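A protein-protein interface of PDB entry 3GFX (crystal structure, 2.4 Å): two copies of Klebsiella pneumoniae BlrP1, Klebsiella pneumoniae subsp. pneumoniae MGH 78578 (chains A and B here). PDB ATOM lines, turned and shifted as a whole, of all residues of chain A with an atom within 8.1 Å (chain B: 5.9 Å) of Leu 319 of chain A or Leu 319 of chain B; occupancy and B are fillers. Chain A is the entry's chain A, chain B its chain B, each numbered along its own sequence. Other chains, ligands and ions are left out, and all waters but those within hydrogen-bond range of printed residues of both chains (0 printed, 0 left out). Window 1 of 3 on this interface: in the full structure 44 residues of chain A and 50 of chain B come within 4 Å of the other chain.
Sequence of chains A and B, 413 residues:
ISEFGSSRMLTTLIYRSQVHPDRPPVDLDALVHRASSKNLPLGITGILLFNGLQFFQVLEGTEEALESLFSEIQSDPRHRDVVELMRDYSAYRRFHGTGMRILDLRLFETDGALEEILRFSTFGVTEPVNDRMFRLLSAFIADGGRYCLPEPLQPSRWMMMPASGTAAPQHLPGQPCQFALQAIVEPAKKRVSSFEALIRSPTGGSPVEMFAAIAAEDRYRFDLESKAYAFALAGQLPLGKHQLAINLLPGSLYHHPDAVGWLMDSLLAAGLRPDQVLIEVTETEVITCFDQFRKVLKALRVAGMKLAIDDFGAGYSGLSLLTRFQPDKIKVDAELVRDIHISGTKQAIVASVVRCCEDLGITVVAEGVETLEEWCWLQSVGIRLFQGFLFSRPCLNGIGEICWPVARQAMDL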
ATOM      1  N   GLU A 283       7.686   4.080 -11.849  1.00  0.00           N
ATOM      2  CA  GLU A 283       8.637   5.131 -11.493  1.00  0.00           C
ATOM      3  C   GLU A 283       9.655   5.389 -12.608  1.00  0.00           C
ATOM      4  O   GLU A 283       9.973   6.541 -12.908  1.00  0.00           O
ATOM      5  CB  GLU A 283       9.363   4.762 -10.195  1.00  0.00           C
ATOM      6  CG  GLU A 283      10.242   5.866  -9.632  1.00  0.00           C
ATOM      7  CD  GLU A 283      11.472   5.327  -8.936  1.00  0.00           C
ATOM      8  OE1 GLU A 283      12.586   5.602  -9.424  1.00  0.00           O
ATOM      9  OE2 GLU A 283      11.330   4.624  -7.914  1.00  0.00           O
ATOM     10  N   ILE A 287       9.825   9.373 -14.703  1.00  0.00           N
ATOM     11  CA  ILE A 287      11.003  10.239 -14.540  1.00  0.00           C
ATOM     12  C   ILE A 287      11.610  10.678 -15.873  1.00  0.00           C
ATOM     13  O   ILE A 287      12.192  11.762 -15.970  1.00  0.00           O
ATOM     14  CB  ILE A 287      12.113   9.582 -13.661  1.00  0.00           C
ATOM     15  CG1 ILE A 287      12.565   8.238 -14.246  1.00  0.00           C
ATOM     16  CG2 ILE A 287      11.647   9.431 -12.220  1.00  0.00           C
ATOM     17  CD1 ILE A 287      13.723   7.582 -13.513  1.00  0.00           C
ATOM     18  N   PHE A 312       7.875   1.427  -7.006  1.00  0.00           N
ATOM     19  CA  PHE A 312       8.545   2.507  -6.288  1.00  0.00           C
ATOM     20  C   PHE A 312       9.843   1.989  -5.681  1.00  0.00           C
ATOM     21  O   PHE A 312       9.830   1.100  -4.824  1.00  0.00           O
ATOM     22  CB  PHE A 312       7.625   3.070  -5.201  1.00  0.00           C
ATOM     23  CG  PHE A 312       8.088   4.382  -4.620  1.00  0.00           C
ATOM     24  CD1 PHE A 312       7.639   5.587  -5.145  1.00  0.00           C
ATOM     25  CD2 PHE A 312       8.955   4.411  -3.531  1.00  0.00           C
ATOM     26  CE1 PHE A 312       8.055   6.795  -4.603  1.00  0.00           C
ATOM     27  CE2 PHE A 312       9.375   5.615  -2.986  1.00  0.00           C
ATOM     28  CZ  PHE A 312       8.921   6.809  -3.520  1.00  0.00           C
ATOM     29  N   GLY A 313      10.959   2.540  -6.151  1.00  0.00           N
ATOM     30  CA  GLY A 313      12.284   2.105  -5.723  1.00  0.00           C
ATOM     31  C   GLY A 313      13.137   1.521  -6.835  1.00  0.00           C
ATOM     32  O   GLY A 313      14.368   1.569  -6.769  1.00  0.00           O
ATOM     33  N   TYR A 316      15.457   3.998  -8.547  1.00  0.00           N
ATOM     34  CA  TYR A 316      16.236   4.746  -7.545  1.00  0.00           C
ATOM     35  C   TYR A 316      15.950   6.255  -7.532  1.00  0.00           C
ATOM     36  O   TYR A 316      16.791   7.050  -7.119  1.00  0.00           O
ATOM     37  CB  TYR A 316      17.743   4.457  -7.674  1.00  0.00           C
ATOM     38  CG  TYR A 316      18.059   3.016  -8.011  1.00  0.00           C
ATOM     39  CD1 TYR A 316      17.930   2.011  -7.056  1.00  0.00           C
ATOM     40  CD2 TYR A 316      18.479   2.657  -9.290  1.00  0.00           C
ATOM     41  CE1 TYR A 316      18.209   0.685  -7.364  1.00  0.00           C
ATOM     42  CE2 TYR A 316      18.760   1.337  -9.609  1.00  0.00           C
ATOM     43  CZ  TYR A 316      18.626   0.356  -8.643  1.00  0.00           C
ATOM     44  OH  TYR A 316      18.908  -0.952  -8.967  1.00  0.00           O
ATOM     45  N   SER A 317      14.752   6.637  -7.965  1.00  0.00           N
ATOM     46  CA  SER A 317      14.401   8.047  -8.115  1.00  0.00           C
ATOM     47  C   SER A 317      13.001   8.339  -7.576  1.00  0.00           C
ATOM     48  O   SER A 317      12.281   9.188  -8.110  1.00  0.00           O
ATOM     49  CB  SER A 317      14.507   8.460  -9.586  1.00  0.00           C
ATOM     50  OG  SER A 317      14.249   9.845  -9.749  1.00  0.00           O
ATOM     51  N   GLY A 318      12.622   7.635  -6.514  1.00  0.00           N
ATOM     52  CA  GLY A 318      11.300   7.793  -5.925  1.00  0.00           C
ATOM     53  C   GLY A 318      11.164   9.030  -5.054  1.00  0.00           C
ATOM     54  O   GLY A 318      10.117   9.679  -5.046  1.00  0.00           O
ATOM     55  N   LEU A 319      12.226   9.345  -4.319  1.00  0.00           N
ATOM     56  CA  LEU A 319      12.249  10.484  -3.404  1.00  0.00           C
ATOM     57  C   LEU A 319      12.138  11.818  -4.141  1.00  0.00           C
ATOM     58  O   LEU A 319      11.422  12.721  -3.705  1.00  0.00           O
ATOM     59  CB  LEU A 319      13.525  10.432  -2.559  1.00  0.00           C
ATOM     60  CG  LEU A 319      13.967  11.632  -1.721  1.00  0.00           C
ATOM     61  CD1 LEU A 319      14.587  11.128  -0.446  1.00  0.00           C
ATOM     62  CD2 LEU A 319      14.946  12.531  -2.470  1.00  0.00           C
ATOM     63  N   SER A 320      12.852  11.929  -5.256  1.00  0.00           N
ATOM     64  CA  SER A 320      12.843  13.141  -6.071  1.00  0.00           C
ATOM     65  C   SER A 320      11.556  13.263  -6.879  1.00  0.00           C
ATOM     66  O   SER A 320      11.209  14.346  -7.354  1.00  0.00           O
ATOM     67  CB  SER A 320      14.047  13.155  -7.011  1.00  0.00           C
ATOM     68  OG  SER A 320      13.988  12.085  -7.940  1.00  0.00           O
ATOM     69  N   LEU A 321      10.861  12.140  -7.038  1.00  0.00           N
ATOM     70  CA  LEU A 321       9.581  12.094  -7.733  1.00  0.00           C
ATOM     71  C   LEU A 321       8.477  12.704  -6.872  1.00  0.00           C
ATOM     72  O   LEU A 321       7.585  13.386  -7.382  1.00  0.00           O
ATOM     73  CB  LEU A 321       9.235  10.646  -8.079  1.00  0.00           C
ATOM     74  CG  LEU A 321       8.088  10.357  -9.044  1.00  0.00           C
ATOM     75  CD1 LEU A 321       8.545  10.538 -10.469  1.00  0.00           C
ATOM     76  CD2 LEU A 321       7.601   8.942  -8.842  1.00  0.00           C
ATOM     77  N   LEU A 322       8.555  12.460  -5.563  1.00  0.00           N
ATOM     78  CA  LEU A 322       7.584  12.982  -4.602  1.00  0.00           C
ATOM     79  C   LEU A 322       7.706  14.495  -4.424  1.00  0.00           C
ATOM     80  O   LEU A 322       6.784  15.146  -3.934  1.00  0.00           O
ATOM     81  CB  LEU A 322       7.723  12.265  -3.256  1.00  0.00           C
ATOM     82  CG  LEU A 322       7.425  10.761  -3.234  1.00  0.00           C
ATOM     83  CD1 LEU A 322       7.879  10.137  -1.923  1.00  0.00           C
ATOM     84  CD2 LEU A 322       5.950  10.476  -3.484  1.00  0.00           C
ATOM     85  N   THR A 323       8.852  15.037  -4.829  1.00  0.00           N
ATOM     86  CA  THR A 323       9.094  16.477  -4.856  1.00  0.00           C
ATOM     87  C   THR A 323       8.244  17.154  -5.933  1.00  0.00           C
ATOM     88  O   THR A 323       7.690  18.234  -5.708  1.00  0.00           O
ATOM     89  CB  THR A 323      10.596  16.767  -5.100  1.00  0.00           C
ATOM     90  OG1 THR A 323      11.355  16.336  -3.964  1.00  0.00           O
ATOM     91  CG2 THR A 323      10.850  18.245  -5.338  1.00  0.00           C
ATOM     92  N   ARG A 324       8.130  16.504  -7.089  1.00  0.00           N
ATOM     93  CA  ARG A 324       7.414  17.062  -8.236  1.00  0.00           C
ATOM     94  C   ARG A 324       5.902  17.010  -8.051  1.00  0.00           C
ATOM     95  O   ARG A 324       5.207  18.002  -8.265  1.00  0.00           O
ATOM     96  CB  ARG A 324       7.791  16.322  -9.525  1.00  0.00           C
ATOM     97  CG  ARG A 324       9.283  16.209  -9.796  1.00  0.00           C
ATOM     98  CD  ARG A 324       9.942  17.569  -9.924  1.00  0.00           C
ATOM     99  NE  ARG A 324      11.271  17.477 -10.522  1.00  0.00           N
ATOM    100  CZ  ARG A 324      12.383  17.177  -9.855  1.00  0.00           C
ATOM    101  NH1 ARG A 324      12.344  16.927  -8.552  1.00  0.00           N
ATOM    102  NH2 ARG A 324      13.542  17.123 -10.498  1.00  0.00           N
ATOM    103  N   PHE A 325       5.403  15.841  -7.662  1.00  0.00           N
ATOM    104  CA  PHE A 325       3.973  15.624  -7.486  1.00  0.00           C
ATOM    105  C   PHE A 325       3.726  14.585  -6.403  1.00  0.00           C
ATOM    106  O   PHE A 325       4.626  13.827  -6.042  1.00  0.00           O
ATOM    107  CB  PHE A 325       3.315  15.193  -8.808  1.00  0.00           C
ATOM    108  CG  PHE A 325       3.780  13.851  -9.318  1.00  0.00           C
ATOM    109  CD1 PHE A 325       4.945  13.741 -10.071  1.00  0.00           C
ATOM    110  CD2 PHE A 325       3.041  12.699  -9.063  1.00  0.00           C
ATOM    111  CE1 PHE A 325       5.375  12.507 -10.545  1.00  0.00           C
ATOM    112  CE2 PHE A 325       3.463  11.461  -9.533  1.00  0.00           C
ATOM    113  CZ  PHE A 325       4.631  11.366 -10.277  1.00  0.00           C
ATOM    114  N   LEU A 336      12.475  -4.733  -3.080  1.00  0.00           N
ATOM    115  CA  LEU A 336      12.628  -4.209  -1.723  1.00  0.00           C
ATOM    116  C   LEU A 336      11.943  -5.106  -0.693  1.00  0.00           C
ATOM    117  O   LEU A 336      12.382  -5.195   0.455  1.00  0.00           O
ATOM    118  CB  LEU A 336      12.090  -2.779  -1.629  1.00  0.00           C
ATOM    119  CG  LEU A 336      12.936  -1.680  -2.281  1.00  0.00           C
ATOM    120  CD1 LEU A 336      12.144  -0.385  -2.402  1.00  0.00           C
ATOM    121  CD2 LEU A 336      14.230  -1.453  -1.511  1.00  0.00           C
ATOM    122  N   THR A 345      19.286  -3.072   5.417  1.00  0.00           N
ATOM    123  CA  THR A 345      19.241  -2.023   4.405  1.00  0.00           C
ATOM    124  C   THR A 345      17.806  -1.786   3.937  1.00  0.00           C
ATOM    125  O   THR A 345      17.297  -0.670   4.043  1.00  0.00           O
ATOM    126  CB  THR A 345      20.143  -2.368   3.192  1.00  0.00           C
ATOM    127  OG1 THR A 345      21.485  -2.597   3.639  1.00  0.00           O
ATOM    128  CG2 THR A 345      20.147  -1.236   2.183  1.00  0.00           C
ATOM    129  N   LYS A 346      17.161  -2.844   3.449  1.00  0.00           N
ATOM    130  CA  LYS A 346      15.784  -2.772   2.949  1.00  0.00           C
ATOM    131  C   LYS A 346      14.772  -2.419   4.041  1.00  0.00           C
ATOM    132  O   LYS A 346      13.789  -1.723   3.777  1.00  0.00           O
ATOM    133  CB  LYS A 346      15.392  -4.081   2.256  1.00  0.00           C
ATOM    134  CG  LYS A 346      16.174  -4.356   0.979  1.00  0.00           C
ATOM    135  CD  LYS A 346      15.837  -5.713   0.383  1.00  0.00           C
ATOM    136  CE  LYS A 346      16.696  -5.996  -0.840  1.00  0.00           C
ATOM    137  NZ  LYS A 346      16.316  -7.268  -1.515  1.00  0.00           N
ATOM    138  N   ALA A 348      15.353  -0.433   6.631  1.00  0.00           N
ATOM    139  CA  ALA A 348      15.495   1.001   6.866  1.00  0.00           C
ATOM    140  C   ALA A 348      14.859   1.837   5.754  1.00  0.00           C
ATOM    141  O   ALA A 348      14.231   2.861   6.028  1.00  0.00           O
ATOM    142  CB  ALA A 348      16.961   1.371   7.042  1.00  0.00           C
ATOM    143  N   ILE A 349      15.020   1.387   4.510  1.00  0.00           N
ATOM    144  CA  ILE A 349      14.480   2.084   3.339  1.00  0.00           C
ATOM    145  C   ILE A 349      12.952   2.062   3.317  1.00  0.00           C
ATOM    146  O   ILE A 349      12.317   3.114   3.212  1.00  0.00           O
ATOM    147  CB  ILE A 349      15.045   1.501   2.021  1.00  0.00           C
ATOM    148  CG1 ILE A 349      16.552   1.744   1.943  1.00  0.00           C
ATOM    149  CG2 ILE A 349      14.357   2.119   0.804  1.00  0.00           C
ATOM    150  CD1 ILE A 349      17.266   0.840   0.976  1.00  0.00           C
ATOM    151  N   VAL A 350      12.375   0.867   3.437  1.00  0.00           N
ATOM    152  CA  VAL A 350      10.921   0.694   3.412  1.00  0.00           C
ATOM    153  C   VAL A 350      10.231   1.445   4.559  1.00  0.00           C
ATOM    154  O   VAL A 350       9.240   2.136   4.333  1.00  0.00           O
ATOM    155  CB  VAL A 350      10.524  -0.808   3.371  1.00  0.00           C
ATOM    156  CG1 VAL A 350       9.027  -0.995   3.577  1.00  0.00           C
ATOM    157  CG2 VAL A 350      10.944  -1.419   2.044  1.00  0.00           C
ATOM    158  N   ALA A 351      10.786   1.338   5.767  1.00  0.00           N
ATOM    159  CA  ALA A 351      10.260   2.047   6.941  1.00  0.00           C
ATOM    160  C   ALA A 351      10.255   3.564   6.760  1.00  0.00           C
ATOM    161  O   ALA A 351       9.341   4.246   7.227  1.00  0.00           O
ATOM    162  CB  ALA A 351      11.046   1.673   8.193  1.00  0.00           C
ATOM    163  N   SER A 352      11.282   4.080   6.089  1.00  0.00           N
ATOM    164  CA  SER A 352      11.372   5.504   5.772  1.00  0.00           C
ATOM    165  C   SER A 352      10.331   5.944   4.749  1.00  0.00           C
ATOM    166  O   SER A 352       9.715   7.001   4.900  1.00  0.00           O
ATOM    167  CB  SER A 352      12.771   5.857   5.273  1.00  0.00           C
ATOM    168  OG  SER A 352      13.492   6.539   6.278  1.00  0.00           O
ATOM    169  N   VAL A 353      10.149   5.128   3.715  1.00  0.00           N
ATOM    170  CA  VAL A 353       9.158   5.376   2.674  1.00  0.00           C
ATOM    171  C   VAL A 353       7.744   5.397   3.268  1.00  0.00           C
ATOM    172  O   VAL A 353       6.971   6.321   3.004  1.00  0.00           O
ATOM    173  CB  VAL A 353       9.289   4.330   1.537  1.00  0.00           C
ATOM    174  CG1 VAL A 353       8.067   4.316   0.656  1.00  0.00           C
ATOM    175  CG2 VAL A 353      10.535   4.604   0.708  1.00  0.00           C
ATOM    176  N   VAL A 354       7.435   4.390   4.087  1.00  0.00           N
ATOM    177  CA  VAL A 354       6.156   4.292   4.796  1.00  0.00           C
ATOM    178  C   VAL A 354       5.890   5.539   5.639  1.00  0.00           C
ATOM    179  O   VAL A 354       4.807   6.127   5.568  1.00  0.00           O
ATOM    180  CB  VAL A 354       6.111   3.031   5.700  1.00  0.00           C
ATOM    181  CG1 VAL A 354       4.869   3.023   6.579  1.00  0.00           C
ATOM    182  CG2 VAL A 354       6.155   1.780   4.858  1.00  0.00           C
ATOM    183  N   CYS A 356       7.324   8.533   5.370  1.00  0.00           N
ATOM    184  CA  CYS A 356       7.214   9.704   4.499  1.00  0.00           C
ATOM    185  C   CYS A 356       5.824   9.808   3.874  1.00  0.00           C
ATOM    186  O   CYS A 356       5.231  10.885   3.845  1.00  0.00           O
ATOM    187  CB  CYS A 356       8.291   9.672   3.411  1.00  0.00           C
ATOM    188  SG  CYS A 356       8.264  11.089   2.294  1.00  0.00           S
ATOM    189  N   LEU A 360       2.579  12.421   4.231  1.00  0.00           N
ATOM    190  CA  LEU A 360       2.073  13.054   3.015  1.00  0.00           C
ATOM    191  C   LEU A 360       0.655  12.611   2.661  1.00  0.00           C
ATOM    192  O   LEU A 360       0.037  13.168   1.756  1.00  0.00           O
ATOM    193  CB  LEU A 360       3.021  12.782   1.842  1.00  0.00           C
ATOM    194  CG  LEU A 360       4.416  13.408   1.915  1.00  0.00           C
ATOM    195  CD1 LEU A 360       5.267  12.966   0.735  1.00  0.00           C
ATOM    196  CD2 LEU A 360       4.325  14.920   1.987  1.00  0.00           C
ATOM    197  N   GLU B 283      24.184  11.226  -7.396  1.00  0.00           N
ATOM    198  CA  GLU B 283      23.489  10.005  -7.799  1.00  0.00           C
ATOM    199  C   GLU B 283      23.245   9.950  -9.309  1.00  0.00           C
ATOM    200  O   GLU B 283      23.321   8.877  -9.907  1.00  0.00           O
ATOM    201  CB  GLU B 283      22.168   9.840  -7.042  1.00  0.00           C
ATOM    202  CG  GLU B 283      21.542   8.465  -7.221  1.00  0.00           C
ATOM    203  CD  GLU B 283      20.119   8.378  -6.708  1.00  0.00           C
ATOM    204  OE1 GLU B 283      19.900   8.531  -5.486  1.00  0.00           O
ATOM    205  OE2 GLU B 283      19.218   8.136  -7.535  1.00  0.00           O
ATOM    206  N   PHE B 312      21.768  15.236  -2.961  1.00  0.00           N
ATOM    207  CA  PHE B 312      20.727  14.234  -2.808  1.00  0.00           C
ATOM    208  C   PHE B 312      19.373  14.920  -2.684  1.00  0.00           C
ATOM    209  O   PHE B 312      19.062  15.538  -1.666  1.00  0.00           O
ATOM    210  CB  PHE B 312      21.009  13.332  -1.604  1.00  0.00           C
ATOM    211  CG  PHE B 312      20.204  12.066  -1.593  1.00  0.00           C
ATOM    212  CD1 PHE B 312      20.507  11.027  -2.463  1.00  0.00           C
ATOM    213  CD2 PHE B 312      19.144  11.913  -0.710  1.00  0.00           C
ATOM    214  CE1 PHE B 312      19.764   9.858  -2.455  1.00  0.00           C
ATOM    215  CE2 PHE B 312      18.396  10.745  -0.696  1.00  0.00           C
ATOM    216  CZ  PHE B 312      18.708   9.718  -1.568  1.00  0.00           C
ATOM    217  N   GLY B 313      18.584  14.809  -3.748  1.00  0.00           N
ATOM    218  CA  GLY B 313      17.335  15.544  -3.888  1.00  0.00           C
ATOM    219  C   GLY B 313      17.198  16.102  -5.293  1.00  0.00           C
ATOM    220  O   GLY B 313      16.090  16.208  -5.819  1.00  0.00           O
ATOM    221  N   SER B 317      17.073  10.892  -7.478  1.00  0.00           N
ATOM    222  CA  SER B 317      17.351  10.733  -6.059  1.00  0.00           C
ATOM    223  C   SER B 317      16.332   9.837  -5.376  1.00  0.00           C
ATOM    224  O   SER B 317      15.127  10.047  -5.490  1.00  0.00           O
ATOM    225  CB  SER B 317      17.408  12.093  -5.363  1.00  0.00           C
ATOM    226  OG  SER B 317      18.625  12.763  -5.654  1.00  0.00           O
ATOM    227  N   GLY B 318      16.833   8.833  -4.668  1.00  0.00           N
ATOM    228  CA  GLY B 318      15.995   7.941  -3.880  1.00  0.00           C
ATOM    229  C   GLY B 318      16.857   7.150  -2.925  1.00  0.00           C
ATOM    230  O   GLY B 318      18.001   6.835  -3.240  1.00  0.00           O
ATOM    231  N   LEU B 319      16.329   6.830  -1.748  1.00  0.00           N
ATOM    232  CA  LEU B 319      17.095   5.990  -0.829  1.00  0.00           C
ATOM    233  C   LEU B 319      17.131   4.490  -1.121  1.00  0.00           C
ATOM    234  O   LEU B 319      17.804   3.742  -0.425  1.00  0.00           O
ATOM    235  CB  LEU B 319      16.905   6.328   0.663  1.00  0.00           C
ATOM    236  CG  LEU B 319      15.602   6.651   1.401  1.00  0.00           C
ATOM    237  CD1 LEU B 319      15.440   8.154   1.544  1.00  0.00           C
ATOM    238  CD2 LEU B 319      14.379   6.009   0.764  1.00  0.00           C
ATOM    239  N   SER B 320      16.434   4.067  -2.174  1.00  0.00           N
ATOM    240  CA  SER B 320      16.544   2.701  -2.693  1.00  0.00           C
ATOM    241  C   SER B 320      17.887   2.495  -3.397  1.00  0.00           C
ATOM    242  O   SER B 320      18.291   1.366  -3.673  1.00  0.00           O
ATOM    243  CB  SER B 320      15.392   2.400  -3.652  1.00  0.00           C
ATOM    244  OG  SER B 320      15.240   3.437  -4.608  1.00  0.00           O
ATOM    245  N   LEU B 321      18.560   3.607  -3.685  1.00  0.00           N
ATOM    246  CA  LEU B 321      19.932   3.627  -4.170  1.00  0.00           C
ATOM    247  C   LEU B 321      20.874   2.991  -3.150  1.00  0.00           C
ATOM    248  O   LEU B 321      21.916   2.445  -3.509  1.00  0.00           O
ATOM    249  CB  LEU B 321      20.336   5.079  -4.431  1.00  0.00           C
ATOM    250  CG  LEU B 321      21.659   5.533  -5.053  1.00  0.00           C
ATOM    251  CD1 LEU B 321      22.728   5.781  -4.000  1.00  0.00           C
ATOM    252  CD2 LEU B 321      22.147   4.600  -6.147  1.00  0.00           C
ATOM    253  N   LEU B 322      20.485   3.057  -1.880  1.00  0.00           N
ATOM    254  CA  LEU B 322      21.281   2.514  -0.783  1.00  0.00           C
ATOM    255  C   LEU B 322      21.340   0.982  -0.752  1.00  0.00           C
ATOM    256  O   LEU B 322      22.101   0.408   0.023  1.00  0.00           O
ATOM    257  CB  LEU B 322      20.809   3.080   0.565  1.00  0.00           C
ATOM    258  CG  LEU B 322      20.861   4.606   0.724  1.00  0.00           C
ATOM    259  CD1 LEU B 322      20.127   5.060   1.974  1.00  0.00           C
ATOM    260  CD2 LEU B 322      22.290   5.104   0.743  1.00  0.00           C
ATOM    261  N   THR B 323      20.551   0.307  -1.596  1.00  0.00           N
ATOM    262  CA  THR B 323      20.629  -1.147  -1.782  1.00  0.00           C
ATOM    263  C   THR B 323      21.828  -1.536  -2.642  1.00  0.00           C
ATOM    264  O   THR B 323      22.303  -2.672  -2.582  1.00  0.00           O
ATOM    265  CB  THR B 323      19.361  -1.725  -2.451  1.00  0.00           C
ATOM    266  OG1 THR B 323      19.107  -1.042  -3.685  1.00  0.00           O
ATOM    267  CG2 THR B 323      18.153  -1.606  -1.540  1.00  0.00           C
ATOM    268  N   LEU B 336      15.768  20.827  -1.702  1.00  0.00           N
ATOM    269  CA  LEU B 336      14.948  20.287  -0.617  1.00  0.00           C
ATOM    270  C   LEU B 336      14.979  21.206   0.604  1.00  0.00           C
ATOM    271  O   LEU B 336      14.005  21.294   1.353  1.00  0.00           O
ATOM    272  CB  LEU B 336      15.405  18.879  -0.225  1.00  0.00           C
ATOM    273  CG  LEU B 336      15.037  17.703  -1.137  1.00  0.00           C
ATOM    274  CD1 LEU B 336      15.662  16.425  -0.606  1.00  0.00           C
ATOM    275  CD2 LEU B 336      13.528  17.539  -1.264  1.00  0.00           C
ATOM    276  N   ILE B 349      10.002  14.531   3.433  1.00  0.00           N
ATOM    277  CA  ILE B 349      11.077  13.911   2.656  1.00  0.00           C
ATOM    278  C   ILE B 349      12.435  13.997   3.364  1.00  0.00           C
ATOM    279  O   ILE B 349      13.142  12.994   3.476  1.00  0.00           O
ATOM    280  CB  ILE B 349      11.153  14.516   1.227  1.00  0.00           C
ATOM    281  CG1 ILE B 349       9.967  14.039   0.383  1.00  0.00           C
ATOM    282  CG2 ILE B 349      12.466  14.157   0.543  1.00  0.00           C
ATOM    283  CD1 ILE B 349       9.746  14.838  -0.884  1.00  0.00           C
ATOM    284  N   SER B 352      12.606  11.861   6.406  1.00  0.00           N
ATOM    285  CA  SER B 352      12.715  10.474   5.979  1.00  0.00           C
ATOM    286  C   SER B 352      14.165  10.094   5.677  1.00  0.00           C
ATOM    287  O   SER B 352      14.593   8.978   5.972  1.00  0.00           O
ATOM    288  CB  SER B 352      11.843  10.244   4.744  1.00  0.00           C
ATOM    289  OG  SER B 352      11.632   8.867   4.515  1.00  0.00           O
ATOM    290  N   VAL B 353      14.905  11.032   5.085  1.00  0.00           N
ATOM    291  CA  VAL B 353      16.329  10.854   4.784  1.00  0.00           C
ATOM    292  C   VAL B 353      17.141  10.744   6.074  1.00  0.00           C
ATOM    293  O   VAL B 353      17.975   9.845   6.219  1.00  0.00           O
ATOM    294  CB  VAL B 353      16.876  12.027   3.922  1.00  0.00           C
ATOM    295  CG1 VAL B 353      18.395  11.959   3.786  1.00  0.00           C
ATOM    296  CG2 VAL B 353      16.229  12.037   2.557  1.00  0.00           C
ATOM    297  N   CYS B 356      16.459   7.322   7.831  1.00  0.00           N
ATOM    298  CA  CYS B 356      17.031   6.201   7.083  1.00  0.00           C
ATOM    299  C   CYS B 356      18.544   6.132   7.253  1.00  0.00           C
ATOM    300  O   CYS B 356      19.106   5.053   7.448  1.00  0.00           O
ATOM    301  CB  CYS B 356      16.683   6.305   5.597  1.00  0.00           C
ATOM    302  SG  CYS B 356      17.201   4.878   4.612  1.00  0.00           S
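Of the 26 printed residues of chain A, 13 touch a printed residue of chain B. Hydrophobic or aromatic side chains of chain A within 4 Å of the printed part of chain B: Tyr 316, Leu 319, Leu 336 and Ile 349. Among the printed residues, 28 pairs touch across the chains. Among the printed residues, no Asp or Glu carboxylate lies within 4 Å of a Lys or Arg side-chain nitrogen of the other chain.
Leu 319 of chain A touches Gly 318 of chain B, but with the chains exchanged Gly 318 of chain A does not touch Leu 319 of chain B (6.1 Å). Leu 319 of chain A touches Ile 349 of chain B, and with the chains exchanged Ile 349 of chain A touches Leu 319 of chain B.
Printed residues of chain B within 4 Å of Gly 318 of chain A: Ser 317. Of chain B, only Phe 312, Ser 317, Gly 318, Leu 319, Ile 349 and Val 353 come within 4 Å of Leu 319 of chain A. Of the printed residues of chain B, Ser 320 of chain A touches Gly 313 and Ser 317. Val 353 of chain A touches none of the printed residues of chain B. Of chain A, only Leu 319 (3.7 Å) and Ile 349 (3.3 Å) come within 4 Å of Leu 319 of chain B. Of the printed residues of chain A, Ser 320 of chain B touches Gly 313 (3.0 Å) and Tyr 316 (3.4 Å). The nearest residue of chain A that does not touch Leu 319 of chain B is Val 353 of chain A (4.1 Å).
The backbone carbonyl oxygen (O) of Gly 313 of chain A is in hydrogen-bond range of the side-chain hydroxyl (OG) of Ser 320 of chain B (3.0 Å). OG of Ser 352 of chain A lies close to N of Cys 356 of chain B, 3.4 Å away. The backbone NH (N) of Leu 319 of chain A is in hydrogen-bond range of the backbone carbonyl oxygen (O) of Ser 317 of chain B. The backbone NH (N) of Gly 318 of chain B lies within hydrogen-bond range of the backbone carbonyl oxygen (O) of Tyr 316 of chain A, at 3.0 Å. The backbone carbonyl oxygen (O) of Tyr 316 of chain A sits close to the side-chain carboxylate (OE2) of Glu 283 of chain B, at 2.7 Å. The backbone carbonyl oxygen of Ser 352 of chain B is in hydrogen-bond range of the side-chain hydroxyl of Ser 352 of chain A (2.7 Å). The backbone NH (N) of Ser 320 of chain A sits at hydrogen-bond distance from the backbone carbonyl oxygen (O) of Ser 317 of chain B.
OE2 of Glu 283 of chain A is in hydrogen-bond range of N of Gly 313 of chain A. The side-chain carboxylate (OE2) of Glu 283 of chain B sits at hydrogen-bond distance from the backbone NH (N) of Ser 317 of chain B (3.5 Å).
Ser 320 of chain B touches Tyr 316 of chain A. Ile 349 of chain B touches Leu 319 of chain A (CG2 to CG, 3.7 Å). CG2 of Thr 323 of chain B touches CD2 of Leu 336 of chain A, at 3.9 Å. Ile 349 of chain A touches Leu 319 of chain B. Cys 356 of chain A touches Ile 349 of chain B (SG to CG1, 3.9 Å).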
